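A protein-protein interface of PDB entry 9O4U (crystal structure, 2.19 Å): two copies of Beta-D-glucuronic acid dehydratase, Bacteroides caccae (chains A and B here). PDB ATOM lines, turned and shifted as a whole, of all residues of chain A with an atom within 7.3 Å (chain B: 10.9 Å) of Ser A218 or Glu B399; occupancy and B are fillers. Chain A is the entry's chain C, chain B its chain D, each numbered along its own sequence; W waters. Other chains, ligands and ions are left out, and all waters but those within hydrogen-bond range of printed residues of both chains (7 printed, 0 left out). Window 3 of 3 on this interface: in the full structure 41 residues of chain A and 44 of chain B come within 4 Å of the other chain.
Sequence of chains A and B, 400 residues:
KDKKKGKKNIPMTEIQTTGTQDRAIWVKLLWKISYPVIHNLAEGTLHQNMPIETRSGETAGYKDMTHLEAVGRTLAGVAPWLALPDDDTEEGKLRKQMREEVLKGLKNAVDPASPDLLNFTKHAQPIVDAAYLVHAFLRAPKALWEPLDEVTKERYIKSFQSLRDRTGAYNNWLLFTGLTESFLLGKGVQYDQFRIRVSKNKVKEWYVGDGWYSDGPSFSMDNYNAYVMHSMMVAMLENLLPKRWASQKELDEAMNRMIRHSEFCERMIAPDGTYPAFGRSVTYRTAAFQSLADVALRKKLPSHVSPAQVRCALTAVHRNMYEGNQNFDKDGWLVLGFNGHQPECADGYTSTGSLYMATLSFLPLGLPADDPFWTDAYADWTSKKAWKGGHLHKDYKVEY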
ATOM      1  N   TYR A 170       2.074  -0.864 -18.012  1.00  0.00           N
ATOM      2  CA  TYR A 170       1.762  -1.641 -16.816  1.00  0.00           C
ATOM      3  C   TYR A 170       2.828  -2.726 -16.650  1.00  0.00           C
ATOM      4  O   TYR A 170       2.599  -3.912 -16.865  1.00  0.00           O
ATOM      5  CB  TYR A 170       0.357  -2.221 -16.927  1.00  0.00           C
ATOM      6  CG  TYR A 170      -0.136  -2.963 -15.702  1.00  0.00           C
ATOM      7  CD1 TYR A 170      -0.299  -2.315 -14.493  1.00  0.00           C
ATOM      8  CD2 TYR A 170      -0.484  -4.302 -15.776  1.00  0.00           C
ATOM      9  CE1 TYR A 170      -0.767  -2.982 -13.388  1.00  0.00           C
ATOM     10  CE2 TYR A 170      -0.954  -4.972 -14.688  1.00  0.00           C
ATOM     11  CZ  TYR A 170      -1.088  -4.306 -13.484  1.00  0.00           C
ATOM     12  OH  TYR A 170      -1.556  -4.971 -12.370  1.00  0.00           O
ATOM     13  N   TRP A 206       4.922  -9.627  -9.216  1.00  0.00           N
ATOM     14  CA  TRP A 206       5.540 -10.080 -10.463  1.00  0.00           C
ATOM     15  C   TRP A 206       6.787 -10.940 -10.272  1.00  0.00           C
ATOM     16  O   TRP A 206       7.375 -11.360 -11.275  1.00  0.00           O
ATOM     17  CB  TRP A 206       5.918  -8.890 -11.339  1.00  0.00           C
ATOM     18  CG  TRP A 206       4.756  -8.255 -11.984  1.00  0.00           C
ATOM     19  CD1 TRP A 206       3.581  -8.856 -12.348  1.00  0.00           C
ATOM     20  CD2 TRP A 206       4.630  -6.874 -12.333  1.00  0.00           C
ATOM     21  NE1 TRP A 206       2.734  -7.925 -12.915  1.00  0.00           N
ATOM     22  CE2 TRP A 206       3.362  -6.703 -12.916  1.00  0.00           C
ATOM     23  CE3 TRP A 206       5.474  -5.765 -12.211  1.00  0.00           C
ATOM     24  CZ2 TRP A 206       2.917  -5.470 -13.374  1.00  0.00           C
ATOM     25  CZ3 TRP A 206       5.034  -4.545 -12.667  1.00  0.00           C
ATOM     26  CH2 TRP A 206       3.763  -4.404 -13.234  1.00  0.00           C
ATOM     27  N   VAL A 208       8.764 -14.069 -10.197  1.00  0.00           N
ATOM     28  CA  VAL A 208       8.408 -15.410 -10.654  1.00  0.00           C
ATOM     29  C   VAL A 208       9.270 -16.471  -9.970  1.00  0.00           C
ATOM     30  O   VAL A 208       8.805 -17.589  -9.732  1.00  0.00           O
ATOM     31  CB  VAL A 208       8.485 -15.525 -12.187  1.00  0.00           C
ATOM     32  CG1 VAL A 208       7.353 -14.700 -12.828  1.00  0.00           C
ATOM     33  CG2 VAL A 208       9.851 -15.104 -12.718  1.00  0.00           C
ATOM     34  N   TYR A 213      11.987 -11.329 -11.942  1.00  0.00           N
ATOM     35  CA  TYR A 213      10.636 -10.800 -12.012  1.00  0.00           C
ATOM     36  C   TYR A 213      10.150 -10.898 -13.452  1.00  0.00           C
ATOM     37  O   TYR A 213      10.948 -10.858 -14.397  1.00  0.00           O
ATOM     38  CB  TYR A 213      10.565  -9.323 -11.595  1.00  0.00           C
ATOM     39  CG  TYR A 213      11.063  -8.939 -10.214  1.00  0.00           C
ATOM     40  CD1 TYR A 213      10.214  -8.976  -9.116  1.00  0.00           C
ATOM     41  CD2 TYR A 213      12.360  -8.466 -10.021  1.00  0.00           C
ATOM     42  CE1 TYR A 213      10.647  -8.600  -7.846  1.00  0.00           C
ATOM     43  CE2 TYR A 213      12.810  -8.075  -8.753  1.00  0.00           C
ATOM     44  CZ  TYR A 213      11.944  -8.149  -7.670  1.00  0.00           C
ATOM     45  OH  TYR A 213      12.365  -7.773  -6.412  1.00  0.00           O
ATOM     46  N   SER A 214       8.831 -11.002 -13.612  1.00  0.00           N
ATOM     47  CA  SER A 214       8.218 -10.716 -14.896  1.00  0.00           C
ATOM     48  C   SER A 214       8.143  -9.207 -15.088  1.00  0.00           C
ATOM     49  O   SER A 214       7.845  -8.454 -14.150  1.00  0.00           O
ATOM     50  CB  SER A 214       6.820 -11.323 -14.987  1.00  0.00           C
ATOM     51  OG  SER A 214       5.970 -10.740 -14.018  1.00  0.00           O
ATOM     52  N   ASP A 215       8.448  -8.768 -16.305  1.00  0.00           N
ATOM     53  CA  ASP A 215       8.383  -7.354 -16.662  1.00  0.00           C
ATOM     54  C   ASP A 215       6.938  -7.053 -17.050  1.00  0.00           C
ATOM     55  O   ASP A 215       6.565  -7.016 -18.229  1.00  0.00           O
ATOM     56  CB  ASP A 215       9.352  -7.049 -17.795  1.00  0.00           C
ATOM     57  CG  ASP A 215       9.391  -5.569 -18.152  1.00  0.00           C
ATOM     58  OD1 ASP A 215       8.750  -4.751 -17.454  1.00  0.00           O
ATOM     59  OD2 ASP A 215      10.085  -5.227 -19.119  1.00  0.00           O
ATOM     60  N   GLY A 216       6.105  -6.837 -16.034  1.00  0.00           N
ATOM     61  CA  GLY A 216       4.677  -6.765 -16.255  1.00  0.00           C
ATOM     62  C   GLY A 216       4.058  -8.136 -16.087  1.00  0.00           C
ATOM     63  O   GLY A 216       4.674  -9.052 -15.540  1.00  0.00           O
ATOM     64  N   PRO A 217       2.820  -8.310 -16.555  1.00  0.00           N
ATOM     65  CA  PRO A 217       2.093  -9.560 -16.260  1.00  0.00           C
ATOM     66  C   PRO A 217       2.718 -10.812 -16.861  1.00  0.00           C
ATOM     67  O   PRO A 217       2.498 -11.906 -16.323  1.00  0.00           O
ATOM     68  CB  PRO A 217       0.698  -9.296 -16.844  1.00  0.00           C
ATOM     69  CG  PRO A 217       0.573  -7.790 -16.812  1.00  0.00           C
ATOM     70  CD  PRO A 217       1.947  -7.291 -17.158  1.00  0.00           C
ATOM     71  N   SER A 218       3.501 -10.692 -17.928  1.00  0.00           N
ATOM     72  CA  SER A 218       4.023 -11.836 -18.663  1.00  0.00           C
ATOM     73  C   SER A 218       5.542 -11.870 -18.554  1.00  0.00           C
ATOM     74  O   SER A 218       6.207 -10.837 -18.719  1.00  0.00           O
ATOM     75  CB  SER A 218       3.589 -11.769 -20.132  1.00  0.00           C
ATOM     76  OG  SER A 218       3.952 -12.945 -20.822  1.00  0.00           O
ATOM     77  N   PHE A 219       6.091 -13.049 -18.262  1.00  0.00           N
ATOM     78  CA  PHE A 219       7.534 -13.149 -18.096  1.00  0.00           C
ATOM     79  C   PHE A 219       8.242 -12.836 -19.401  1.00  0.00           C
ATOM     80  O   PHE A 219       7.837 -13.298 -20.471  1.00  0.00           O
ATOM     81  CB  PHE A 219       7.950 -14.537 -17.626  1.00  0.00           C
ATOM     82  CG  PHE A 219       9.433 -14.662 -17.406  1.00  0.00           C
ATOM     83  CD1 PHE A 219      10.040 -14.040 -16.320  1.00  0.00           C
ATOM     84  CD2 PHE A 219      10.226 -15.380 -18.295  1.00  0.00           C
ATOM     85  CE1 PHE A 219      11.393 -14.144 -16.120  1.00  0.00           C
ATOM     86  CE2 PHE A 219      11.586 -15.485 -18.091  1.00  0.00           C
ATOM     87  CZ  PHE A 219      12.161 -14.874 -16.996  1.00  0.00           C
ATOM     88  N   SER A 220       9.316 -12.054 -19.302  1.00  0.00           N
ATOM     89  CA  SER A 220      10.088 -11.626 -20.459  1.00  0.00           C
ATOM     90  C   SER A 220      11.547 -11.993 -20.220  1.00  0.00           C
ATOM     91  O   SER A 220      12.165 -11.499 -19.272  1.00  0.00           O
ATOM     92  CB  SER A 220       9.942 -10.120 -20.686  1.00  0.00           C
ATOM     93  OG  SER A 220       8.582  -9.725 -20.590  1.00  0.00           O
ATOM     94  N   MET A 221      12.095 -12.854 -21.074  1.00  0.00           N
ATOM     95  CA  MET A 221      13.499 -13.242 -20.970  1.00  0.00           C
ATOM     96  C   MET A 221      14.327 -12.171 -21.672  1.00  0.00           C
ATOM     97  O   MET A 221      14.591 -12.231 -22.875  1.00  0.00           O
ATOM     98  CB  MET A 221      13.708 -14.633 -21.561  1.00  0.00           C
ATOM     99  CG  MET A 221      15.095 -15.221 -21.357  1.00  0.00           C
ATOM    100  SD  MET A 221      15.962 -14.787 -19.818  1.00  0.00           S
ATOM    101  CE  MET A 221      14.921 -15.494 -18.606  1.00  0.00           C
ATOM    102  N   TRP B 206       2.105 -23.795 -15.458  1.00  0.00           N
ATOM    103  CA  TRP B 206       3.433 -23.293 -15.113  1.00  0.00           C
ATOM    104  C   TRP B 206       4.056 -22.401 -16.195  1.00  0.00           C
ATOM    105  O   TRP B 206       5.134 -21.845 -15.963  1.00  0.00           O
ATOM    106  CB  TRP B 206       4.367 -24.466 -14.778  1.00  0.00           C
ATOM    107  CG  TRP B 206       4.109 -25.084 -13.408  1.00  0.00           C
ATOM    108  CD1 TRP B 206       3.577 -24.456 -12.308  1.00  0.00           C
ATOM    109  CD2 TRP B 206       4.341 -26.451 -13.004  1.00  0.00           C
ATOM    110  NE1 TRP B 206       3.499 -25.335 -11.249  1.00  0.00           N
ATOM    111  CE2 TRP B 206       3.950 -26.563 -11.651  1.00  0.00           C
ATOM    112  CE3 TRP B 206       4.847 -27.579 -13.651  1.00  0.00           C
ATOM    113  CZ2 TRP B 206       4.038 -27.753 -10.942  1.00  0.00           C
ATOM    114  CZ3 TRP B 206       4.939 -28.761 -12.948  1.00  0.00           C
ATOM    115  CH2 TRP B 206       4.532 -28.840 -11.606  1.00  0.00           C
ATOM    116  N   TYR B 207       3.417 -22.225 -17.356  1.00  0.00           N
ATOM    117  CA  TYR B 207       3.932 -21.261 -18.336  1.00  0.00           C
ATOM    118  C   TYR B 207       3.941 -19.847 -17.758  1.00  0.00           C
ATOM    119  O   TYR B 207       2.928 -19.372 -17.246  1.00  0.00           O
ATOM    120  CB  TYR B 207       3.094 -21.282 -19.602  1.00  0.00           C
ATOM    121  CG  TYR B 207       3.724 -20.514 -20.747  1.00  0.00           C
ATOM    122  CD1 TYR B 207       4.842 -21.020 -21.403  1.00  0.00           C
ATOM    123  CD2 TYR B 207       3.209 -19.288 -21.163  1.00  0.00           C
ATOM    124  CE1 TYR B 207       5.433 -20.335 -22.447  1.00  0.00           C
ATOM    125  CE2 TYR B 207       3.789 -18.590 -22.221  1.00  0.00           C
ATOM    126  CZ  TYR B 207       4.899 -19.128 -22.864  1.00  0.00           C
ATOM    127  OH  TYR B 207       5.499 -18.468 -23.913  1.00  0.00           O
ATOM    128  N   VAL B 208       5.090 -19.176 -17.819  1.00  0.00           N
ATOM    129  CA  VAL B 208       5.193 -17.825 -17.275  1.00  0.00           C
ATOM    130  C   VAL B 208       5.334 -16.755 -18.349  1.00  0.00           C
ATOM    131  O   VAL B 208       4.976 -15.596 -18.087  1.00  0.00           O
ATOM    132  CB  VAL B 208       6.341 -17.712 -16.249  1.00  0.00           C
ATOM    133  CG1 VAL B 208       6.036 -18.582 -15.042  1.00  0.00           C
ATOM    134  CG2 VAL B 208       7.683 -18.080 -16.887  1.00  0.00           C
ATOM    135  N   GLY B 209       5.796 -17.090 -19.540  1.00  0.00           N
ATOM    136  CA  GLY B 209       5.829 -16.147 -20.643  1.00  0.00           C
ATOM    137  C   GLY B 209       7.098 -16.244 -21.470  1.00  0.00           C
ATOM    138  O   GLY B 209       8.117 -16.787 -21.045  1.00  0.00           O
ATOM    139  N   ASP B 210       7.022 -15.709 -22.692  1.00  0.00           N
ATOM    140  CA  ASP B 210       8.179 -15.541 -23.572  1.00  0.00           C
ATOM    141  C   ASP B 210       8.930 -16.847 -23.827  1.00  0.00           C
ATOM    142  O   ASP B 210      10.153 -16.849 -23.987  1.00  0.00           O
ATOM    143  CB  ASP B 210       9.137 -14.490 -23.024  1.00  0.00           C
ATOM    144  CG  ASP B 210      10.005 -13.898 -24.096  1.00  0.00           C
ATOM    145  OD1 ASP B 210       9.602 -13.961 -25.283  1.00  0.00           O
ATOM    146  OD2 ASP B 210      11.085 -13.387 -23.745  1.00  0.00           O
ATOM    147  N   GLY B 211       8.207 -17.963 -23.885  1.00  0.00           N
ATOM    148  CA  GLY B 211       8.784 -19.257 -24.180  1.00  0.00           C
ATOM    149  C   GLY B 211       9.319 -20.023 -22.989  1.00  0.00           C
ATOM    150  O   GLY B 211      10.043 -21.005 -23.183  1.00  0.00           O
ATOM    151  N   TRP B 212       8.985 -19.624 -21.772  1.00  0.00           N
ATOM    152  CA  TRP B 212       9.535 -20.252 -20.581  1.00  0.00           C
ATOM    153  C   TRP B 212       8.422 -20.748 -19.674  1.00  0.00           C
ATOM    154  O   TRP B 212       7.420 -20.058 -19.475  1.00  0.00           O
ATOM    155  CB  TRP B 212      10.416 -19.277 -19.813  1.00  0.00           C
ATOM    156  CG  TRP B 212      11.662 -18.953 -20.504  1.00  0.00           C
ATOM    157  CD1 TRP B 212      11.829 -18.062 -21.520  1.00  0.00           C
ATOM    158  CD2 TRP B 212      12.952 -19.518 -20.241  1.00  0.00           C
ATOM    159  NE1 TRP B 212      13.150 -18.032 -21.905  1.00  0.00           N
ATOM    160  CE2 TRP B 212      13.862 -18.916 -21.137  1.00  0.00           C
ATOM    161  CE3 TRP B 212      13.430 -20.463 -19.323  1.00  0.00           C
ATOM    162  CZ2 TRP B 212      15.220 -19.237 -21.154  1.00  0.00           C
ATOM    163  CZ3 TRP B 212      14.772 -20.786 -19.344  1.00  0.00           C
ATOM    164  CH2 TRP B 212      15.654 -20.167 -20.248  1.00  0.00           C
ATOM    165  N   TYR B 213       8.615 -21.954 -19.137  1.00  0.00           N
ATOM    166  CA  TYR B 213       7.842 -22.501 -18.035  1.00  0.00           C
ATOM    167  C   TYR B 213       8.655 -22.421 -16.748  1.00  0.00           C
ATOM    168  O   TYR B 213       9.886 -22.494 -16.767  1.00  0.00           O
ATOM    169  CB  TYR B 213       7.498 -23.977 -18.247  1.00  0.00           C
ATOM    170  CG  TYR B 213       6.754 -24.368 -19.501  1.00  0.00           C
ATOM    171  CD1 TYR B 213       5.379 -24.436 -19.511  1.00  0.00           C
ATOM    172  CD2 TYR B 213       7.438 -24.746 -20.647  1.00  0.00           C
ATOM    173  CE1 TYR B 213       4.686 -24.830 -20.646  1.00  0.00           C
ATOM    174  CE2 TYR B 213       6.762 -25.150 -21.787  1.00  0.00           C
ATOM    175  CZ  TYR B 213       5.377 -25.185 -21.782  1.00  0.00           C
ATOM    176  OH  TYR B 213       4.672 -25.581 -22.907  1.00  0.00           O
ATOM    177  N   PHE B 219       9.744 -20.249 -10.629  1.00  0.00           N
ATOM    178  CA  PHE B 219      10.561 -20.117 -11.828  1.00  0.00           C
ATOM    179  C   PHE B 219      12.028 -20.425 -11.536  1.00  0.00           C
ATOM    180  O   PHE B 219      12.599 -19.952 -10.548  1.00  0.00           O
ATOM    181  CB  PHE B 219      10.449 -18.714 -12.418  1.00  0.00           C
ATOM    182  CG  PHE B 219      11.232 -18.554 -13.692  1.00  0.00           C
ATOM    183  CD1 PHE B 219      10.828 -19.206 -14.849  1.00  0.00           C
ATOM    184  CD2 PHE B 219      12.377 -17.780 -13.733  1.00  0.00           C
ATOM    185  CE1 PHE B 219      11.537 -19.078 -16.023  1.00  0.00           C
ATOM    186  CE2 PHE B 219      13.093 -17.647 -14.914  1.00  0.00           C
ATOM    187  CZ  PHE B 219      12.663 -18.296 -16.058  1.00  0.00           C
ATOM    188  N   GLU B 253       0.141 -24.092 -29.512  1.00  0.00           N
ATOM    189  CA  GLU B 253       0.673 -23.273 -28.426  1.00  0.00           C
ATOM    190  C   GLU B 253       2.010 -23.815 -27.918  1.00  0.00           C
ATOM    191  O   GLU B 253       3.005 -23.088 -27.838  1.00  0.00           O
ATOM    192  CB  GLU B 253      -0.357 -23.232 -27.300  1.00  0.00           C
ATOM    193  CG  GLU B 253      -0.030 -22.338 -26.143  1.00  0.00           C
ATOM    194  CD  GLU B 253      -1.173 -22.292 -25.158  1.00  0.00           C
ATOM    195  OE1 GLU B 253      -1.596 -23.369 -24.679  1.00  0.00           O
ATOM    196  OE2 GLU B 253      -1.666 -21.181 -24.880  1.00  0.00           O
ATOM    197  N   ASN B 256       4.757 -23.449 -30.581  1.00  0.00           N
ATOM    198  CA  ASN B 256       5.251 -22.084 -30.731  1.00  0.00           C
ATOM    199  C   ASN B 256       6.063 -21.642 -29.519  1.00  0.00           C
ATOM    200  O   ASN B 256       7.011 -20.862 -29.653  1.00  0.00           O
ATOM    201  CB  ASN B 256       4.078 -21.129 -30.960  1.00  0.00           C
ATOM    202  CG  ASN B 256       3.521 -21.225 -32.363  1.00  0.00           C
ATOM    203  OD1 ASN B 256       4.272 -21.312 -33.328  1.00  0.00           O
ATOM    204  ND2 ASN B 256       2.197 -21.216 -32.481  1.00  0.00           N
ATOM    205  N   ARG B 257       5.689 -22.103 -28.327  1.00  0.00           N
ATOM    206  CA  ARG B 257       6.467 -21.778 -27.143  1.00  0.00           C
ATOM    207  C   ARG B 257       7.860 -22.398 -27.220  1.00  0.00           C
ATOM    208  O   ARG B 257       8.850 -21.752 -26.859  1.00  0.00           O
ATOM    209  CB  ARG B 257       5.691 -22.219 -25.902  1.00  0.00           C
ATOM    210  CG  ARG B 257       4.449 -21.356 -25.706  1.00  0.00           C
ATOM    211  CD  ARG B 257       3.456 -21.867 -24.674  1.00  0.00           C
ATOM    212  NE  ARG B 257       2.535 -20.793 -24.305  1.00  0.00           N
ATOM    213  CZ  ARG B 257       1.512 -20.918 -23.468  1.00  0.00           C
ATOM    214  NH1 ARG B 257       1.207 -22.080 -22.917  1.00  0.00           N
ATOM    215  NH2 ARG B 257       0.778 -19.844 -23.176  1.00  0.00           N
ATOM    216  N   ARG B 260       9.806 -20.400 -29.751  1.00  0.00           N
ATOM    217  CA  ARG B 260      10.285 -19.196 -29.081  1.00  0.00           C
ATOM    218  C   ARG B 260      11.484 -19.517 -28.203  1.00  0.00           C
ATOM    219  O   ARG B 260      12.537 -18.874 -28.307  1.00  0.00           O
ATOM    220  CB  ARG B 260       9.172 -18.550 -28.250  1.00  0.00           C
ATOM    221  CG  ARG B 260       9.628 -17.339 -27.436  1.00  0.00           C
ATOM    222  CD  ARG B 260      10.357 -16.309 -28.326  1.00  0.00           C
ATOM    223  NE  ARG B 260      10.836 -15.167 -27.557  1.00  0.00           N
ATOM    224  CZ  ARG B 260      11.729 -14.278 -27.980  1.00  0.00           C
ATOM    225  NH1 ARG B 260      12.275 -14.356 -29.186  1.00  0.00           N
ATOM    226  NH2 ARG B 260      12.091 -13.288 -27.166  1.00  0.00           N
ATOM    227  N   GLU B 263      14.933 -19.659 -29.700  1.00  0.00           N
ATOM    228  CA  GLU B 263      15.597 -18.430 -30.099  1.00  0.00           C
ATOM    229  C   GLU B 263      16.601 -18.009 -29.050  1.00  0.00           C
ATOM    230  O   GLU B 263      17.743 -17.679 -29.369  1.00  0.00           O
ATOM    231  CB  GLU B 263      14.579 -17.324 -30.329  1.00  0.00           C
ATOM    232  CG  GLU B 263      13.803 -17.464 -31.605  1.00  0.00           C
ATOM    233  CD  GLU B 263      13.034 -16.199 -31.923  1.00  0.00           C
ATOM    234  OE1 GLU B 263      13.577 -15.317 -32.611  1.00  0.00           O
ATOM    235  OE2 GLU B 263      11.897 -16.073 -31.446  1.00  0.00           O
ATOM    236  N   ASP B 395      15.145  -8.410 -31.313  1.00  0.00           N
ATOM    237  CA  ASP B 395      14.395  -9.334 -30.478  1.00  0.00           C
ATOM    238  C   ASP B 395      13.381  -8.577 -29.623  1.00  0.00           C
ATOM    239  O   ASP B 395      13.538  -7.390 -29.333  1.00  0.00           O
ATOM    240  CB  ASP B 395      15.336 -10.151 -29.587  1.00  0.00           C
ATOM    241  CG  ASP B 395      14.693 -11.425 -29.084  1.00  0.00           C
ATOM    242  OD1 ASP B 395      13.781 -11.942 -29.765  1.00  0.00           O
ATOM    243  OD2 ASP B 395      15.092 -11.913 -28.011  1.00  0.00           O
ATOM    244  N   TYR B 396      12.333  -9.290 -29.220  1.00  0.00           N
ATOM    245  CA  TYR B 396      11.256  -8.715 -28.425  1.00  0.00           C
ATOM    246  C   TYR B 396      10.472  -9.858 -27.786  1.00  0.00           C
ATOM    247  O   TYR B 396      10.155 -10.846 -28.454  1.00  0.00           O
ATOM    248  CB  TYR B 396      10.334  -7.831 -29.294  1.00  0.00           C
ATOM    249  CG  TYR B 396       9.824  -6.613 -28.554  1.00  0.00           C
ATOM    250  CD1 TYR B 396       8.707  -6.692 -27.735  1.00  0.00           C
ATOM    251  CD2 TYR B 396      10.479  -5.391 -28.653  1.00  0.00           C
ATOM    252  CE1 TYR B 396       8.248  -5.582 -27.040  1.00  0.00           C
ATOM    253  CE2 TYR B 396      10.023  -4.275 -27.962  1.00  0.00           C
ATOM    254  CZ  TYR B 396       8.909  -4.379 -27.160  1.00  0.00           C
ATOM    255  OH  TYR B 396       8.456  -3.279 -26.472  1.00  0.00           O
ATOM    256  N   LYS B 397      10.163  -9.726 -26.498  1.00  0.00           N
ATOM    257  CA  LYS B 397       9.440 -10.794 -25.825  1.00  0.00           C
ATOM    258  C   LYS B 397       8.046 -10.946 -26.436  1.00  0.00           C
ATOM    259  O   LYS B 397       7.434  -9.976 -26.894  1.00  0.00           O
ATOM    260  CB  LYS B 397       9.353 -10.537 -24.313  1.00  0.00           C
ATOM    261  CG  LYS B 397       8.267  -9.560 -23.863  1.00  0.00           C
ATOM    262  CD  LYS B 397       8.561  -8.127 -24.324  1.00  0.00           C
ATOM    263  CE  LYS B 397       7.612  -7.165 -23.640  1.00  0.00           C
ATOM    264  NZ  LYS B 397       7.642  -7.383 -22.181  1.00  0.00           N
ATOM    265  N   VAL B 398       7.559 -12.189 -26.466  1.00  0.00           N
ATOM    266  CA  VAL B 398       6.293 -12.512 -27.098  1.00  0.00           C
ATOM    267  C   VAL B 398       5.212 -12.622 -26.030  1.00  0.00           C
ATOM    268  O   VAL B 398       5.482 -12.842 -24.844  1.00  0.00           O
ATOM    269  CB  VAL B 398       6.382 -13.811 -27.944  1.00  0.00           C
ATOM    270  CG1 VAL B 398       7.438 -13.665 -29.028  1.00  0.00           C
ATOM    271  CG2 VAL B 398       6.682 -15.012 -27.070  1.00  0.00           C
ATOM    272  N   GLU B 399       3.958 -12.467 -26.459  1.00  0.00           N
ATOM    273  CA  GLU B 399       2.821 -12.524 -25.546  1.00  0.00           C
ATOM    274  C   GLU B 399       2.104 -13.869 -25.561  1.00  0.00           C
ATOM    275  O   GLU B 399       1.193 -14.081 -24.756  1.00  0.00           O
ATOM    276  CB  GLU B 399       1.829 -11.397 -25.873  1.00  0.00           C
ATOM    277  CG  GLU B 399       2.420 -10.010 -25.681  1.00  0.00           C
ATOM    278  CD  GLU B 399       2.936  -9.785 -24.255  1.00  0.00           C
ATOM    279  OE1 GLU B 399       2.369 -10.351 -23.293  1.00  0.00           O
ATOM    280  OE2 GLU B 399       3.918  -9.045 -24.092  1.00  0.00           O
ATOM    281  N   TYR B 400       2.481 -14.775 -26.452  1.00  0.00           N
ATOM    282  CA  TYR B 400       1.928 -16.113 -26.422  1.00  0.00           C
ATOM    283  C   TYR B 400       2.848 -17.031 -25.620  1.00  0.00           C
ATOM    284  O   TYR B 400       2.598 -18.230 -25.566  1.00  0.00           O
ATOM    285  CB  TYR B 400       1.730 -16.646 -27.844  1.00  0.00           C
ATOM    286  CG  TYR B 400       3.001 -16.669 -28.656  1.00  0.00           C
ATOM    287  CD1 TYR B 400       3.872 -17.745 -28.580  1.00  0.00           C
ATOM    288  CD2 TYR B 400       3.335 -15.614 -29.505  1.00  0.00           C
ATOM    289  CE1 TYR B 400       5.041 -17.776 -29.317  1.00  0.00           C
ATOM    290  CE2 TYR B 400       4.506 -15.639 -30.252  1.00  0.00           C
ATOM    291  CZ  TYR B 400       5.356 -16.727 -30.147  1.00  0.00           C
ATOM    292  OH  TYR B 400       6.526 -16.787 -30.868  1.00  0.00           O
HETATM  293  O   HOH W   1       4.455 -14.929 -23.379  1.00  0.00           O
HETATM  294  O   HOH W   2      12.663 -11.482 -24.784  1.00  0.00           O
HETATM  295  O   HOH W   3       6.233 -11.975 -22.142  1.00  0.00           O
HETATM  296  O   HOH W   4       6.351  -5.460 -20.608  1.00  0.00           O
HETATM  297  O   HOH W   5       5.409  -9.393 -21.716  1.00  0.00           O
HETATM  298  O   HOH W   6      10.389  -6.738 -21.257  1.00  0.00           O
HETATM  299  O   HOH W   7       1.952 -14.858 -21.464  1.00  0.00           O
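The backbone carbonyl oxygen (O) of Val A208 is in hydrogen-bond range of the backbone NH (N) of Phe B219, 3.0 Å away. N of Phe A219 sits at hydrogen-bond distance from O of Val B208, at 2.8 Å. The backbone NH of Asp B210 sits close to the backbone carbonyl oxygen of Phe A219, 3.4 Å away. OG of Ser A220 is in hydrogen-bond range of NZ of Lys B397, at 3.0 Å. N of Met A221 sits at hydrogen-bond distance from OD2 of Asp B210 (2.9 Å).
Of chain B, only Val B208 (3.8 Å), Gly B209 (3.7 Å) and Glu B399 (3.7 Å) come within 4 Å of Ser A218. Glu B399 touches just one residue of chain A: Ser A218 (3.7 Å). No residue of chain B comes within 4 Å of Ser A214. No residue of chain B comes within 4 Å of Asp A215. No residue of chain B comes within 4 Å of Gly A216. Of the printed residues of chain B, Ser A220 touches Asp B210 (3.8 Å) and Lys B397 (3.0 Å). Of the printed residues of chain A, Lys B397 touches Ser A220 (3.0 Å). Printed residues of chain B within 4 Å of Met A221: Asp B210 (2.9 Å) and Trp B212 (3.5 Å). Tyr B207 touches none of the printed residues of chain A. The nearest residue of chain B that does not touch Ser A218 is Val B398 (4.3 Å).
Of the 20 printed residues of chain B, 7 touch a printed residue of chain A. Printed residues of chain B that touch a printed residue of chain A: Val B208, Gly B209, Asp B210, Trp B212, Phe B219, Lys B397 and Glu B399. Hydrophobic or aromatic side chains of chain B that line the printed part of chain A: Val B208, Trp B212 and Phe B219. Of the 12 printed residues of chain A, 5 touch a printed residue of chain B. Along chain A the printed residues that touch a printed residue of chain B span positions 208 to 221. Among the printed residues, no Asp or Glu carboxylate lies within 4 Å of a Lys or Arg side-chain nitrogen of the other chain.
Water W6 lies within hydrogen-bond range of OD2 of Asp A215 (2.6 Å) and NZ of Lys B397 (3.0 Å). Water W1 lies within hydrogen-bond range of O of Val B398 (2.7 Å), N of Asp B210 (2.8 Å) and OG of Ser A218 (3.3 Å).
The side-chain hydroxyl (OH) of Tyr B207 is in hydrogen-bond range of the backbone NH (N) of Asp B210. The guanidinium group (NE) of Arg B260 is in salt-bridge range of the side-chain carboxylate (OD1) of Asp B210 (2.9 Å). The backbone NH (N) of Val B398 is in hydrogen-bond range of the side-chain carboxylate (OD1) of Asp B210, at 3.0 Å.
Among the printed residues, pairs that only touch across the chains: Ser A218 with Val B208 (3.8 Å), Ser A218 with Gly B209 (3.7 Å), Ser A218 with Glu B399 (3.7 Å), Phe A219 with Gly B209 (3.2 Å), Phe A219 with Phe B219 (3.6 Å), Ser A220 with Asp B210 (3.8 Å) and Met A221 with Trp B212 (3.5 Å).
Val A208 touches Phe B219, and with the chains exchanged Phe A219 touches Val B208. Phe B219 touches its own counterpart, Phe A219. Positions printed for both chains: 206, 208, 213 and 219. Of the 12 pairs that touch across the chains among the printed residues, 3 have their exchanged pair printed and touching as well.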
